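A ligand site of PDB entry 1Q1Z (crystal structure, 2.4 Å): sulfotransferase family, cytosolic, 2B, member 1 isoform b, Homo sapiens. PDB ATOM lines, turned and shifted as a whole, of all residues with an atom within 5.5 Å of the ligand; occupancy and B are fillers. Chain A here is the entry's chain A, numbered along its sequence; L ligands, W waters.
The indole nitrogen of Trp 62 lies close to a nitrogen (N3) of the ligand, at 3.2 Å.
Merely in contact with the ligand: Leu 260, Phe 259, Phe 233, Gln 201 and Thr 232.
Hydrophobic or aromatic side chains within 4 Å of the ligand: Trp 62, Tyr 197, Phe 233, Met 236, Phe 259 and Leu 260.
Of the 26 residues printed, 19 come within 4 Å of the ligand.
OG1 of Thr 60 lies within hydrogen-bond range of OG1 of Thr 54 (2.6 Å).
O of Val 264 is in hydrogen-bond range of NH2 of Arg 134 (3.0 Å).
The side-chain hydroxyl (OG1) of Thr 61 is in hydrogen-bond range of the side-chain hydroxyl (OH) of Tyr 244 (3.2 Å).
The indole nitrogen (NE1) of Trp 62 lies within hydrogen-bond range of the backbone carbonyl oxygen (O) of Ser 231 (3.1 Å).
The backbone carbonyl oxygen of Gly 263 sits at hydrogen-bond distance from the side-chain amide nitrogen of Gln 201 (2.8 Å).
OH of Tyr 197 sits at hydrogen-bond distance from NH2 of Arg 134, at 3.4 Å.
The side-chain amide nitrogen of Gln 201 is in hydrogen-bond range of the side-chain hydroxyl of Tyr 197 (3.2 Å).
The side-chain hydroxyl of Tyr 197 sits at hydrogen-bond distance from the backbone NH of Val 264, 3.4 Å away.
O of Ser 231 sits at hydrogen-bond distance from N3 of the ligand (2.9 Å).
O5 of the ligand sits at hydrogen-bond distance from OG1 of Thr 61 (3.2 Å).
The side-chain hydroxyl (OG1) of Thr 60 sits at hydrogen-bond distance from an oxygen (O4) of the ligand (2.7 Å).
The guanidinium group (NH2) of Arg 134 is in salt-bridge range of an oxygen (O3) of the ligand, at 3.1 Å.
The backbone NH of Gly 263 sits at hydrogen-bond distance from an oxygen (O2) of the ligand, at 2.8 Å.
N of Lys 57 sits at hydrogen-bond distance from O4 of the ligand (3.2 Å).
N3 of the ligand sits at hydrogen-bond distance from SD of Met 236.
The backbone NH (N) of Thr 60 sits at hydrogen-bond distance from an oxygen (O4) of the ligand (2.7 Å).
The backbone NH (N) of Gly 59 sits at hydrogen-bond distance from an oxygen (O4) of the ligand (3.1 Å).
An oxygen (O1) of the ligand sits at hydrogen-bond distance from the side-chain hydroxyl of Ser 142, 2.7 Å away.
N of Lys 262 lies within hydrogen-bond range of O2 of the ligand, 2.7 Å away.
N of Thr 61 lies within hydrogen-bond range of O5 of the ligand (3.0 Å).
The backbone NH of Ser 58 lies within hydrogen-bond range of an oxygen (O4) of the ligand, 3.4 Å away.
The guanidinium group (NE) of Arg 261 is in salt-bridge range of an oxygen (O1) of the ligand, 2.9 Å away.
OH of Tyr 197 sits at hydrogen-bond distance from N5 of the ligand (2.7 Å).
An oxygen (O6) of the ligand is in salt-bridge range of the side-chain amino group of Lys 57 (3.1 Å).
Water W2 bridges an oxygen (O1) of the ligand (2.8 Å) and the backbone carbonyl oxygen of Ser 142 (2.9 Å).
Water W4 lies within hydrogen-bond range of O5 of the ligand (2.9 Å), OG1 of Thr 61 (3.4 Å) and OH of Tyr 244 (3.4 Å).
Water W5 lies within hydrogen-bond range of the backbone NH of Val 264 (2.8 Å), an oxygen (O3) of the ligand (2.9 Å) and the backbone NH of Gly 263 (3.2 Å).
Water W3 bridges N of Phe 233 (2.8 Å) and N4 of the ligand (2.9 Å).
Water W1 lies within hydrogen-bond range of O of Asp 138 (2.8 Å), O3 of the ligand (3.0 Å), NH2 of Arg 261 (3.3 Å) and NH2 of Arg 134 (3.3 Å).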
ATOM      1  N   THR A  54     -13.709  36.932  16.929  1.00  0.00           N
ATOM      2  CA  THR A  54     -13.705  35.666  17.651  1.00  0.00           C
ATOM      3  C   THR A  54     -14.088  35.903  19.106  1.00  0.00           C
ATOM      4  O   THR A  54     -14.103  37.036  19.591  1.00  0.00           O
ATOM      5  CB  THR A  54     -12.315  35.025  17.706  1.00  0.00           C
ATOM      6  OG1 THR A  54     -11.435  35.880  18.442  1.00  0.00           O
ATOM      7  CG2 THR A  54     -11.750  34.808  16.323  1.00  0.00           C
ATOM      8  N   TYR A  55     -14.417  34.814  19.785  1.00  0.00           N
ATOM      9  CA  TYR A  55     -14.670  34.867  21.211  1.00  0.00           C
ATOM     10  C   TYR A  55     -13.234  34.610  21.660  1.00  0.00           C
ATOM     11  O   TYR A  55     -12.553  33.747  21.101  1.00  0.00           O
ATOM     12  CB  TYR A  55     -15.586  33.724  21.661  1.00  0.00           C
ATOM     13  CG  TYR A  55     -15.944  33.761  23.123  1.00  0.00           C
ATOM     14  CD1 TYR A  55     -16.966  34.577  23.596  1.00  0.00           C
ATOM     15  CD2 TYR A  55     -15.223  32.999  24.057  1.00  0.00           C
ATOM     16  CE1 TYR A  55     -17.282  34.629  24.950  1.00  0.00           C
ATOM     17  CE2 TYR A  55     -15.519  33.051  25.413  1.00  0.00           C
ATOM     18  CZ  TYR A  55     -16.548  33.870  25.857  1.00  0.00           C
ATOM     19  OH  TYR A  55     -16.821  33.940  27.189  1.00  0.00           O
ATOM     20  N   PRO A  56     -12.731  35.350  22.642  1.00  0.00           N
ATOM     21  CA  PRO A  56     -11.362  35.156  23.135  1.00  0.00           C
ATOM     22  C   PRO A  56     -10.917  33.700  23.374  1.00  0.00           C
ATOM     23  O   PRO A  56     -11.675  32.878  23.873  1.00  0.00           O
ATOM     24  CB  PRO A  56     -11.337  35.987  24.405  1.00  0.00           C
ATOM     25  CG  PRO A  56     -12.278  37.112  24.078  1.00  0.00           C
ATOM     26  CD  PRO A  56     -13.422  36.378  23.427  1.00  0.00           C
ATOM     27  N   LYS A  57      -9.660  33.429  23.014  1.00  0.00           N
ATOM     28  CA  LYS A  57      -9.016  32.122  23.151  1.00  0.00           C
ATOM     29  C   LYS A  57      -9.434  31.100  22.108  1.00  0.00           C
ATOM     30  O   LYS A  57      -9.177  29.909  22.266  1.00  0.00           O
ATOM     31  CB  LYS A  57      -9.248  31.517  24.550  1.00  0.00           C
ATOM     32  CG  LYS A  57      -9.146  32.474  25.729  1.00  0.00           C
ATOM     33  CD  LYS A  57      -7.965  33.444  25.645  1.00  0.00           C
ATOM     34  CE  LYS A  57      -6.626  32.739  25.550  1.00  0.00           C
ATOM     35  NZ  LYS A  57      -5.523  33.726  25.353  1.00  0.00           N
ATOM     36  N   SER A  58     -10.089  31.540  21.029  1.00  0.00           N
ATOM     37  CA  SER A  58     -10.520  30.602  19.995  1.00  0.00           C
ATOM     38  C   SER A  58      -9.466  30.457  18.904  1.00  0.00           C
ATOM     39  O   SER A  58      -9.649  29.691  17.947  1.00  0.00           O
ATOM     40  CB  SER A  58     -11.841  31.048  19.373  1.00  0.00           C
ATOM     41  OG  SER A  58     -12.878  31.151  20.332  1.00  0.00           O
ATOM     42  N   GLY A  59      -8.365  31.190  19.048  1.00  0.00           N
ATOM     43  CA  GLY A  59      -7.295  31.134  18.056  1.00  0.00           C
ATOM     44  C   GLY A  59      -7.154  32.390  17.219  1.00  0.00           C
ATOM     45  O   GLY A  59      -6.721  32.333  16.078  1.00  0.00           O
ATOM     46  N   THR A  60      -7.541  33.534  17.787  1.00  0.00           N
ATOM     47  CA  THR A  60      -7.457  34.815  17.090  1.00  0.00           C
ATOM     48  C   THR A  60      -6.057  34.974  16.510  1.00  0.00           C
ATOM     49  O   THR A  60      -5.879  35.247  15.316  1.00  0.00           O
ATOM     50  CB  THR A  60      -7.719  35.983  18.053  1.00  0.00           C
ATOM     51  OG1 THR A  60      -8.871  35.700  18.867  1.00  0.00           O
ATOM     52  CG2 THR A  60      -7.938  37.268  17.273  1.00  0.00           C
ATOM     53  N   THR A  61      -5.074  34.821  17.381  1.00  0.00           N
ATOM     54  CA  THR A  61      -3.668  34.926  17.025  1.00  0.00           C
ATOM     55  C   THR A  61      -3.372  34.092  15.775  1.00  0.00           C
ATOM     56  O   THR A  61      -2.795  34.603  14.818  1.00  0.00           O
ATOM     57  CB  THR A  61      -2.781  34.448  18.204  1.00  0.00           C
ATOM     58  OG1 THR A  61      -2.700  35.484  19.190  1.00  0.00           O
ATOM     59  CG2 THR A  61      -1.379  34.125  17.725  1.00  0.00           C
ATOM     60  N   TRP A  62      -3.772  32.828  15.788  1.00  0.00           N
ATOM     61  CA  TRP A  62      -3.529  31.957  14.650  1.00  0.00           C
ATOM     62  C   TRP A  62      -3.994  32.622  13.353  1.00  0.00           C
ATOM     63  O   TRP A  62      -3.242  32.715  12.379  1.00  0.00           O
ATOM     64  CB  TRP A  62      -4.268  30.631  14.832  1.00  0.00           C
ATOM     65  CG  TRP A  62      -3.742  29.508  14.010  1.00  0.00           C
ATOM     66  CD1 TRP A  62      -2.761  29.571  13.066  1.00  0.00           C
ATOM     67  CD2 TRP A  62      -4.136  28.129  14.088  1.00  0.00           C
ATOM     68  NE1 TRP A  62      -2.509  28.321  12.564  1.00  0.00           N
ATOM     69  CE2 TRP A  62      -3.338  27.412  13.173  1.00  0.00           C
ATOM     70  CE3 TRP A  62      -5.079  27.426  14.853  1.00  0.00           C
ATOM     71  CZ2 TRP A  62      -3.451  26.032  12.995  1.00  0.00           C
ATOM     72  CZ3 TRP A  62      -5.192  26.046  14.675  1.00  0.00           C
ATOM     73  CH2 TRP A  62      -4.385  25.365  13.758  1.00  0.00           C
ATOM     74  N   HIS A 112     -13.425  41.291  19.503  1.00  0.00           N
ATOM     75  CA  HIS A 112     -14.025  40.195  20.265  1.00  0.00           C
ATOM     76  C   HIS A 112     -15.461  40.555  20.595  1.00  0.00           C
ATOM     77  O   HIS A 112     -16.176  39.784  21.226  1.00  0.00           O
ATOM     78  CB  HIS A 112     -13.279  39.940  21.570  1.00  0.00           C
ATOM     79  CG  HIS A 112     -11.962  39.259  21.390  1.00  0.00           C
ATOM     80  ND1 HIS A 112     -11.796  38.188  20.542  1.00  0.00           N
ATOM     81  CD2 HIS A 112     -10.764  39.461  21.968  1.00  0.00           C
ATOM     82  CE1 HIS A 112     -10.553  37.761  20.599  1.00  0.00           C
ATOM     83  NE2 HIS A 112      -9.906  38.528  21.464  1.00  0.00           N
ATOM     84  N   ARG A 134     -14.142  28.008  18.111  1.00  0.00           N
ATOM     85  CA  ARG A 134     -13.358  26.923  18.654  1.00  0.00           C
ATOM     86  C   ARG A 134     -14.262  26.170  19.618  1.00  0.00           C
ATOM     87  O   ARG A 134     -15.288  26.688  20.019  1.00  0.00           O
ATOM     88  CB  ARG A 134     -12.141  27.461  19.419  1.00  0.00           C
ATOM     89  CG  ARG A 134     -11.129  26.395  19.811  1.00  0.00           C
ATOM     90  CD  ARG A 134      -9.978  26.961  20.621  1.00  0.00           C
ATOM     91  NE  ARG A 134      -8.959  25.943  20.847  1.00  0.00           N
ATOM     92  CZ  ARG A 134      -7.857  26.125  21.570  1.00  0.00           C
ATOM     93  NH1 ARG A 134      -7.622  27.301  22.145  1.00  0.00           N
ATOM     94  NH2 ARG A 134      -7.001  25.139  21.711  1.00  0.00           N
ATOM     95  N   ASP A 138     -12.436  23.649  24.997  1.00  0.00           N
ATOM     96  CA  ASP A 138     -11.029  23.994  24.849  1.00  0.00           C
ATOM     97  C   ASP A 138     -10.819  25.481  25.122  1.00  0.00           C
ATOM     98  O   ASP A 138      -9.783  25.875  25.656  1.00  0.00           O
ATOM     99  CB  ASP A 138     -10.520  23.634  23.458  1.00  0.00           C
ATOM    100  CG  ASP A 138     -10.319  22.144  23.294  1.00  0.00           C
ATOM    101  OD1 ASP A 138      -9.970  21.481  24.278  1.00  0.00           O
ATOM    102  OD2 ASP A 138     -10.490  21.626  22.167  1.00  0.00           O
ATOM    103  N   SER A 142      -8.094  27.086  27.785  1.00  0.00           N
ATOM    104  CA  SER A 142      -7.168  28.121  27.359  1.00  0.00           C
ATOM    105  C   SER A 142      -7.394  29.401  28.161  1.00  0.00           C
ATOM    106  O   SER A 142      -6.443  30.053  28.580  1.00  0.00           O
ATOM    107  CB  SER A 142      -7.339  28.400  25.869  1.00  0.00           C
ATOM    108  OG  SER A 142      -6.402  29.376  25.451  1.00  0.00           O
ATOM    109  N   TYR A 197     -11.199  26.504  14.529  1.00  0.00           N
ATOM    110  CA  TYR A 197      -9.893  26.110  15.005  1.00  0.00           C
ATOM    111  C   TYR A 197      -9.646  24.656  14.600  1.00  0.00           C
ATOM    112  O   TYR A 197      -8.528  24.280  14.241  1.00  0.00           O
ATOM    113  CB  TYR A 197      -9.868  26.240  16.535  1.00  0.00           C
ATOM    114  CG  TYR A 197      -8.535  25.970  17.186  1.00  0.00           C
ATOM    115  CD1 TYR A 197      -7.637  27.015  17.453  1.00  0.00           C
ATOM    116  CD2 TYR A 197      -8.168  24.681  17.552  1.00  0.00           C
ATOM    117  CE1 TYR A 197      -6.412  26.765  18.074  1.00  0.00           C
ATOM    118  CE2 TYR A 197      -6.954  24.423  18.177  1.00  0.00           C
ATOM    119  CZ  TYR A 197      -6.085  25.462  18.433  1.00  0.00           C
ATOM    120  OH  TYR A 197      -4.891  25.209  19.064  1.00  0.00           O
ATOM    121  N   GLN A 201      -6.637  23.041  12.423  1.00  0.00           N
ATOM    122  CA  GLN A 201      -5.818  21.974  13.008  1.00  0.00           C
ATOM    123  C   GLN A 201      -5.792  20.756  12.091  1.00  0.00           C
ATOM    124  O   GLN A 201      -4.796  20.051  12.002  1.00  0.00           O
ATOM    125  CB  GLN A 201      -6.376  21.572  14.382  1.00  0.00           C
ATOM    126  CG  GLN A 201      -5.965  22.476  15.517  1.00  0.00           C
ATOM    127  CD  GLN A 201      -4.550  22.225  15.972  1.00  0.00           C
ATOM    128  OE1 GLN A 201      -3.790  21.513  15.303  1.00  0.00           O
ATOM    129  NE2 GLN A 201      -4.160  22.816  17.095  1.00  0.00           N
ATOM    130  N   SER A 231       2.845  29.636   9.778  1.00  0.00           N
ATOM    131  CA  SER A 231       1.572  29.662  10.522  1.00  0.00           C
ATOM    132  C   SER A 231       1.483  28.555  11.569  1.00  0.00           C
ATOM    133  O   SER A 231       0.590  28.561  12.432  1.00  0.00           O
ATOM    134  CB  SER A 231       0.383  29.530   9.581  1.00  0.00           C
ATOM    135  OG  SER A 231      -0.046  30.795   9.148  1.00  0.00           O
ATOM    136  N   THR A 232       2.396  27.598  11.476  1.00  0.00           N
ATOM    137  CA  THR A 232       2.423  26.474  12.397  1.00  0.00           C
ATOM    138  C   THR A 232       2.682  26.954  13.823  1.00  0.00           C
ATOM    139  O   THR A 232       3.386  27.933  14.039  1.00  0.00           O
ATOM    140  CB  THR A 232       3.484  25.474  11.986  1.00  0.00           C
ATOM    141  OG1 THR A 232       3.287  25.141  10.606  1.00  0.00           O
ATOM    142  CG2 THR A 232       3.396  24.201  12.805  1.00  0.00           C
ATOM    143  N   PHE A 233       2.070  26.249  14.774  1.00  0.00           N
ATOM    144  CA  PHE A 233       2.213  26.584  16.184  1.00  0.00           C
ATOM    145  C   PHE A 233       3.673  26.768  16.582  1.00  0.00           C
ATOM    146  O   PHE A 233       4.029  27.766  17.199  1.00  0.00           O
ATOM    147  CB  PHE A 233       1.583  25.476  17.042  1.00  0.00           C
ATOM    148  CG  PHE A 233       1.680  25.730  18.523  1.00  0.00           C
ATOM    149  CD1 PHE A 233       0.800  26.597  19.154  1.00  0.00           C
ATOM    150  CD2 PHE A 233       2.669  25.113  19.274  1.00  0.00           C
ATOM    151  CE1 PHE A 233       0.899  26.834  20.533  1.00  0.00           C
ATOM    152  CE2 PHE A 233       2.779  25.344  20.647  1.00  0.00           C
ATOM    153  CZ  PHE A 233       1.879  26.211  21.275  1.00  0.00           C
ATOM    154  N   MET A 236       5.268  29.774  15.104  1.00  0.00           N
ATOM    155  CA  MET A 236       4.766  30.943  15.791  1.00  0.00           C
ATOM    156  C   MET A 236       5.285  31.099  17.213  1.00  0.00           C
ATOM    157  O   MET A 236       5.632  32.213  17.621  1.00  0.00           O
ATOM    158  CB  MET A 236       3.236  30.967  15.783  1.00  0.00           C
ATOM    159  CG  MET A 236       2.615  31.478  14.472  1.00  0.00           C
ATOM    160  SD  MET A 236       0.796  31.622  14.498  1.00  0.00           S
ATOM    161  CE  MET A 236       0.612  33.091  15.413  1.00  0.00           C
ATOM    162  N   TYR A 244       3.903  37.220  21.900  1.00  0.00           N
ATOM    163  CA  TYR A 244       3.599  38.073  23.044  1.00  0.00           C
ATOM    164  C   TYR A 244       4.660  38.225  24.131  1.00  0.00           C
ATOM    165  O   TYR A 244       4.363  38.730  25.205  1.00  0.00           O
ATOM    166  CB  TYR A 244       2.291  37.603  23.689  1.00  0.00           C
ATOM    167  CG  TYR A 244       1.062  37.823  22.835  1.00  0.00           C
ATOM    168  CD1 TYR A 244       0.281  38.966  22.965  1.00  0.00           C
ATOM    169  CD2 TYR A 244       0.705  36.896  21.854  1.00  0.00           C
ATOM    170  CE1 TYR A 244      -0.820  39.194  22.148  1.00  0.00           C
ATOM    171  CE2 TYR A 244      -0.396  37.102  21.041  1.00  0.00           C
ATOM    172  CZ  TYR A 244      -1.159  38.258  21.189  1.00  0.00           C
ATOM    173  OH  TYR A 244      -2.252  38.457  20.383  1.00  0.00           O
ATOM    174  N   PHE A 259       1.562  32.779  26.226  1.00  0.00           N
ATOM    175  CA  PHE A 259       0.305  33.052  25.518  1.00  0.00           C
ATOM    176  C   PHE A 259      -0.014  31.852  24.630  1.00  0.00           C
ATOM    177  O   PHE A 259      -1.143  31.385  24.579  1.00  0.00           O
ATOM    178  CB  PHE A 259       0.442  34.293  24.629  1.00  0.00           C
ATOM    179  CG  PHE A 259      -0.864  34.770  24.049  1.00  0.00           C
ATOM    180  CD1 PHE A 259      -1.574  35.813  24.640  1.00  0.00           C
ATOM    181  CD2 PHE A 259      -1.395  34.151  22.927  1.00  0.00           C
ATOM    182  CE1 PHE A 259      -2.795  36.222  24.125  1.00  0.00           C
ATOM    183  CE2 PHE A 259      -2.616  34.568  22.406  1.00  0.00           C
ATOM    184  CZ  PHE A 259      -3.316  35.603  23.005  1.00  0.00           C
ATOM    185  N   LEU A 260       0.998  31.379  23.897  1.00  0.00           N
ATOM    186  CA  LEU A 260       0.846  30.212  23.031  1.00  0.00           C
ATOM    187  C   LEU A 260       1.193  29.007  23.906  1.00  0.00           C
ATOM    188  O   LEU A 260       2.314  28.512  23.898  1.00  0.00           O
ATOM    189  CB  LEU A 260       1.805  30.304  21.829  1.00  0.00           C
ATOM    190  CG  LEU A 260       1.630  31.547  20.935  1.00  0.00           C
ATOM    191  CD1 LEU A 260       2.608  31.529  19.772  1.00  0.00           C
ATOM    192  CD2 LEU A 260       0.208  31.593  20.411  1.00  0.00           C
ATOM    193  N   ARG A 261       0.184  28.559  24.651  1.00  0.00           N
ATOM    194  CA  ARG A 261       0.265  27.460  25.625  1.00  0.00           C
ATOM    195  C   ARG A 261       0.547  26.054  25.072  1.00  0.00           C
ATOM    196  O   ARG A 261       1.638  25.521  25.257  1.00  0.00           O
ATOM    197  CB  ARG A 261      -1.016  27.462  26.451  1.00  0.00           C
ATOM    198  CG  ARG A 261      -1.003  26.706  27.759  1.00  0.00           C
ATOM    199  CD  ARG A 261      -2.352  26.881  28.427  1.00  0.00           C
ATOM    200  NE  ARG A 261      -3.421  26.327  27.605  1.00  0.00           N
ATOM    201  CZ  ARG A 261      -3.733  25.038  27.560  1.00  0.00           C
ATOM    202  NH1 ARG A 261      -3.059  24.167  28.303  1.00  0.00           N
ATOM    203  NH2 ARG A 261      -4.710  24.619  26.772  1.00  0.00           N
ATOM    204  N   LYS A 262      -0.463  25.436  24.450  1.00  0.00           N
ATOM    205  CA  LYS A 262      -0.303  24.089  23.897  1.00  0.00           C
ATOM    206  C   LYS A 262      -0.575  24.029  22.406  1.00  0.00           C
ATOM    207  O   LYS A 262       0.101  23.308  21.670  1.00  0.00           O
ATOM    208  CB  LYS A 262      -1.242  23.100  24.607  1.00  0.00           C
ATOM    209  CG  LYS A 262      -0.585  22.277  25.669  1.00  0.00           C
ATOM    210  CD  LYS A 262      -1.468  21.108  26.106  1.00  0.00           C
ATOM    211  CE  LYS A 262      -0.882  20.422  27.320  1.00  0.00           C
ATOM    212  NZ  LYS A 262      -1.709  19.273  27.786  1.00  0.00           N
ATOM    213  N   GLY A 263      -1.573  24.788  21.965  1.00  0.00           N
ATOM    214  CA  GLY A 263      -1.907  24.795  20.553  1.00  0.00           C
ATOM    215  C   GLY A 263      -2.432  23.492  19.988  1.00  0.00           C
ATOM    216  O   GLY A 263      -2.063  23.102  18.872  1.00  0.00           O
ATOM    217  N   VAL A 264      -3.283  22.787  20.742  1.00  0.00           N
ATOM    218  CA  VAL A 264      -3.866  21.554  20.229  1.00  0.00           C
ATOM    219  C   VAL A 264      -5.362  21.530  20.470  1.00  0.00           C
ATOM    220  O   VAL A 264      -5.936  22.466  21.049  1.00  0.00           O
ATOM    221  CB  VAL A 264      -3.296  20.300  20.929  1.00  0.00           C
ATOM    222  CG1 VAL A 264      -1.816  20.181  20.684  1.00  0.00           C
ATOM    223  CG2 VAL A 264      -3.586  20.359  22.409  1.00  0.00           C
HETATM  224  P1  LIG L   1      -4.180  27.085  23.988  1.00  0.00           P
HETATM  225  O1  LIG L   1      -4.213  27.865  25.238  1.00  0.00           O
HETATM  226  O2  LIG L   1      -2.837  26.602  23.705  1.00  0.00           O
HETATM  227  O3  LIG L   1      -5.127  25.985  23.988  1.00  0.00           O
HETATM  228  P2  LIG L   1      -6.479  33.751  21.160  1.00  0.00           P
HETATM  229  O4  LIG L   1      -7.778  33.910  20.499  1.00  0.00           O
HETATM  230  O5  LIG L   1      -5.405  34.224  20.275  1.00  0.00           O
HETATM  231  O6  LIG L   1      -6.453  34.458  22.451  1.00  0.00           O
HETATM  232  O7  LIG L   1      -6.265  32.198  21.420  1.00  0.00           O
HETATM  233  C1  LIG L   1      -5.059  31.632  21.929  1.00  0.00           C
HETATM  234  C2  LIG L   1      -5.124  30.122  21.719  1.00  0.00           C
HETATM  235  O8  LIG L   1      -4.867  29.853  20.311  1.00  0.00           O
HETATM  236  C3  LIG L   1      -4.070  29.315  22.476  1.00  0.00           C
HETATM  237  O9  LIG L   1      -4.635  28.045  22.792  1.00  0.00           O
HETATM  238  C4  LIG L   1      -2.967  29.271  21.453  1.00  0.00           C
HETATM  239  O10 LIG L   1      -1.946  28.336  21.640  1.00  0.00           O
HETATM  240  C5  LIG L   1      -3.764  28.977  20.206  1.00  0.00           C
HETATM  241  N1  LIG L   1      -2.951  29.212  19.012  1.00  0.00           N
HETATM  242  C6  LIG L   1      -2.349  30.370  18.572  1.00  0.00           C
HETATM  243  N2  LIG L   1      -1.676  30.247  17.464  1.00  0.00           N
HETATM  244  C7  LIG L   1      -1.835  28.910  17.143  1.00  0.00           C
HETATM  245  C8  LIG L   1      -1.359  28.113  16.068  1.00  0.00           C
HETATM  246  N3  LIG L   1      -0.599  28.582  15.105  1.00  0.00           N
HETATM  247  N4  LIG L   1      -1.713  26.791  16.043  1.00  0.00           N
HETATM  248  C9  LIG L   1      -2.495  26.289  17.028  1.00  0.00           C
HETATM  249  N5  LIG L   1      -3.007  26.943  18.097  1.00  0.00           N
HETATM  250  C10 LIG L   1      -2.629  28.255  18.095  1.00  0.00           C
HETATM  251  O   HOH W   1      -7.501  24.509  24.955  1.00  0.00           O
HETATM  252  O   HOH W   2      -3.846  29.861  27.209  1.00  0.00           O
HETATM  253  O   HOH W   3      -0.370  24.909  14.238  1.00  0.00           O
HETATM  254  O   HOH W   4      -5.363  37.072  20.549  1.00  0.00           O
HETATM  255  O   HOH W   5      -4.119  23.361  23.369  1.00  0.00           O
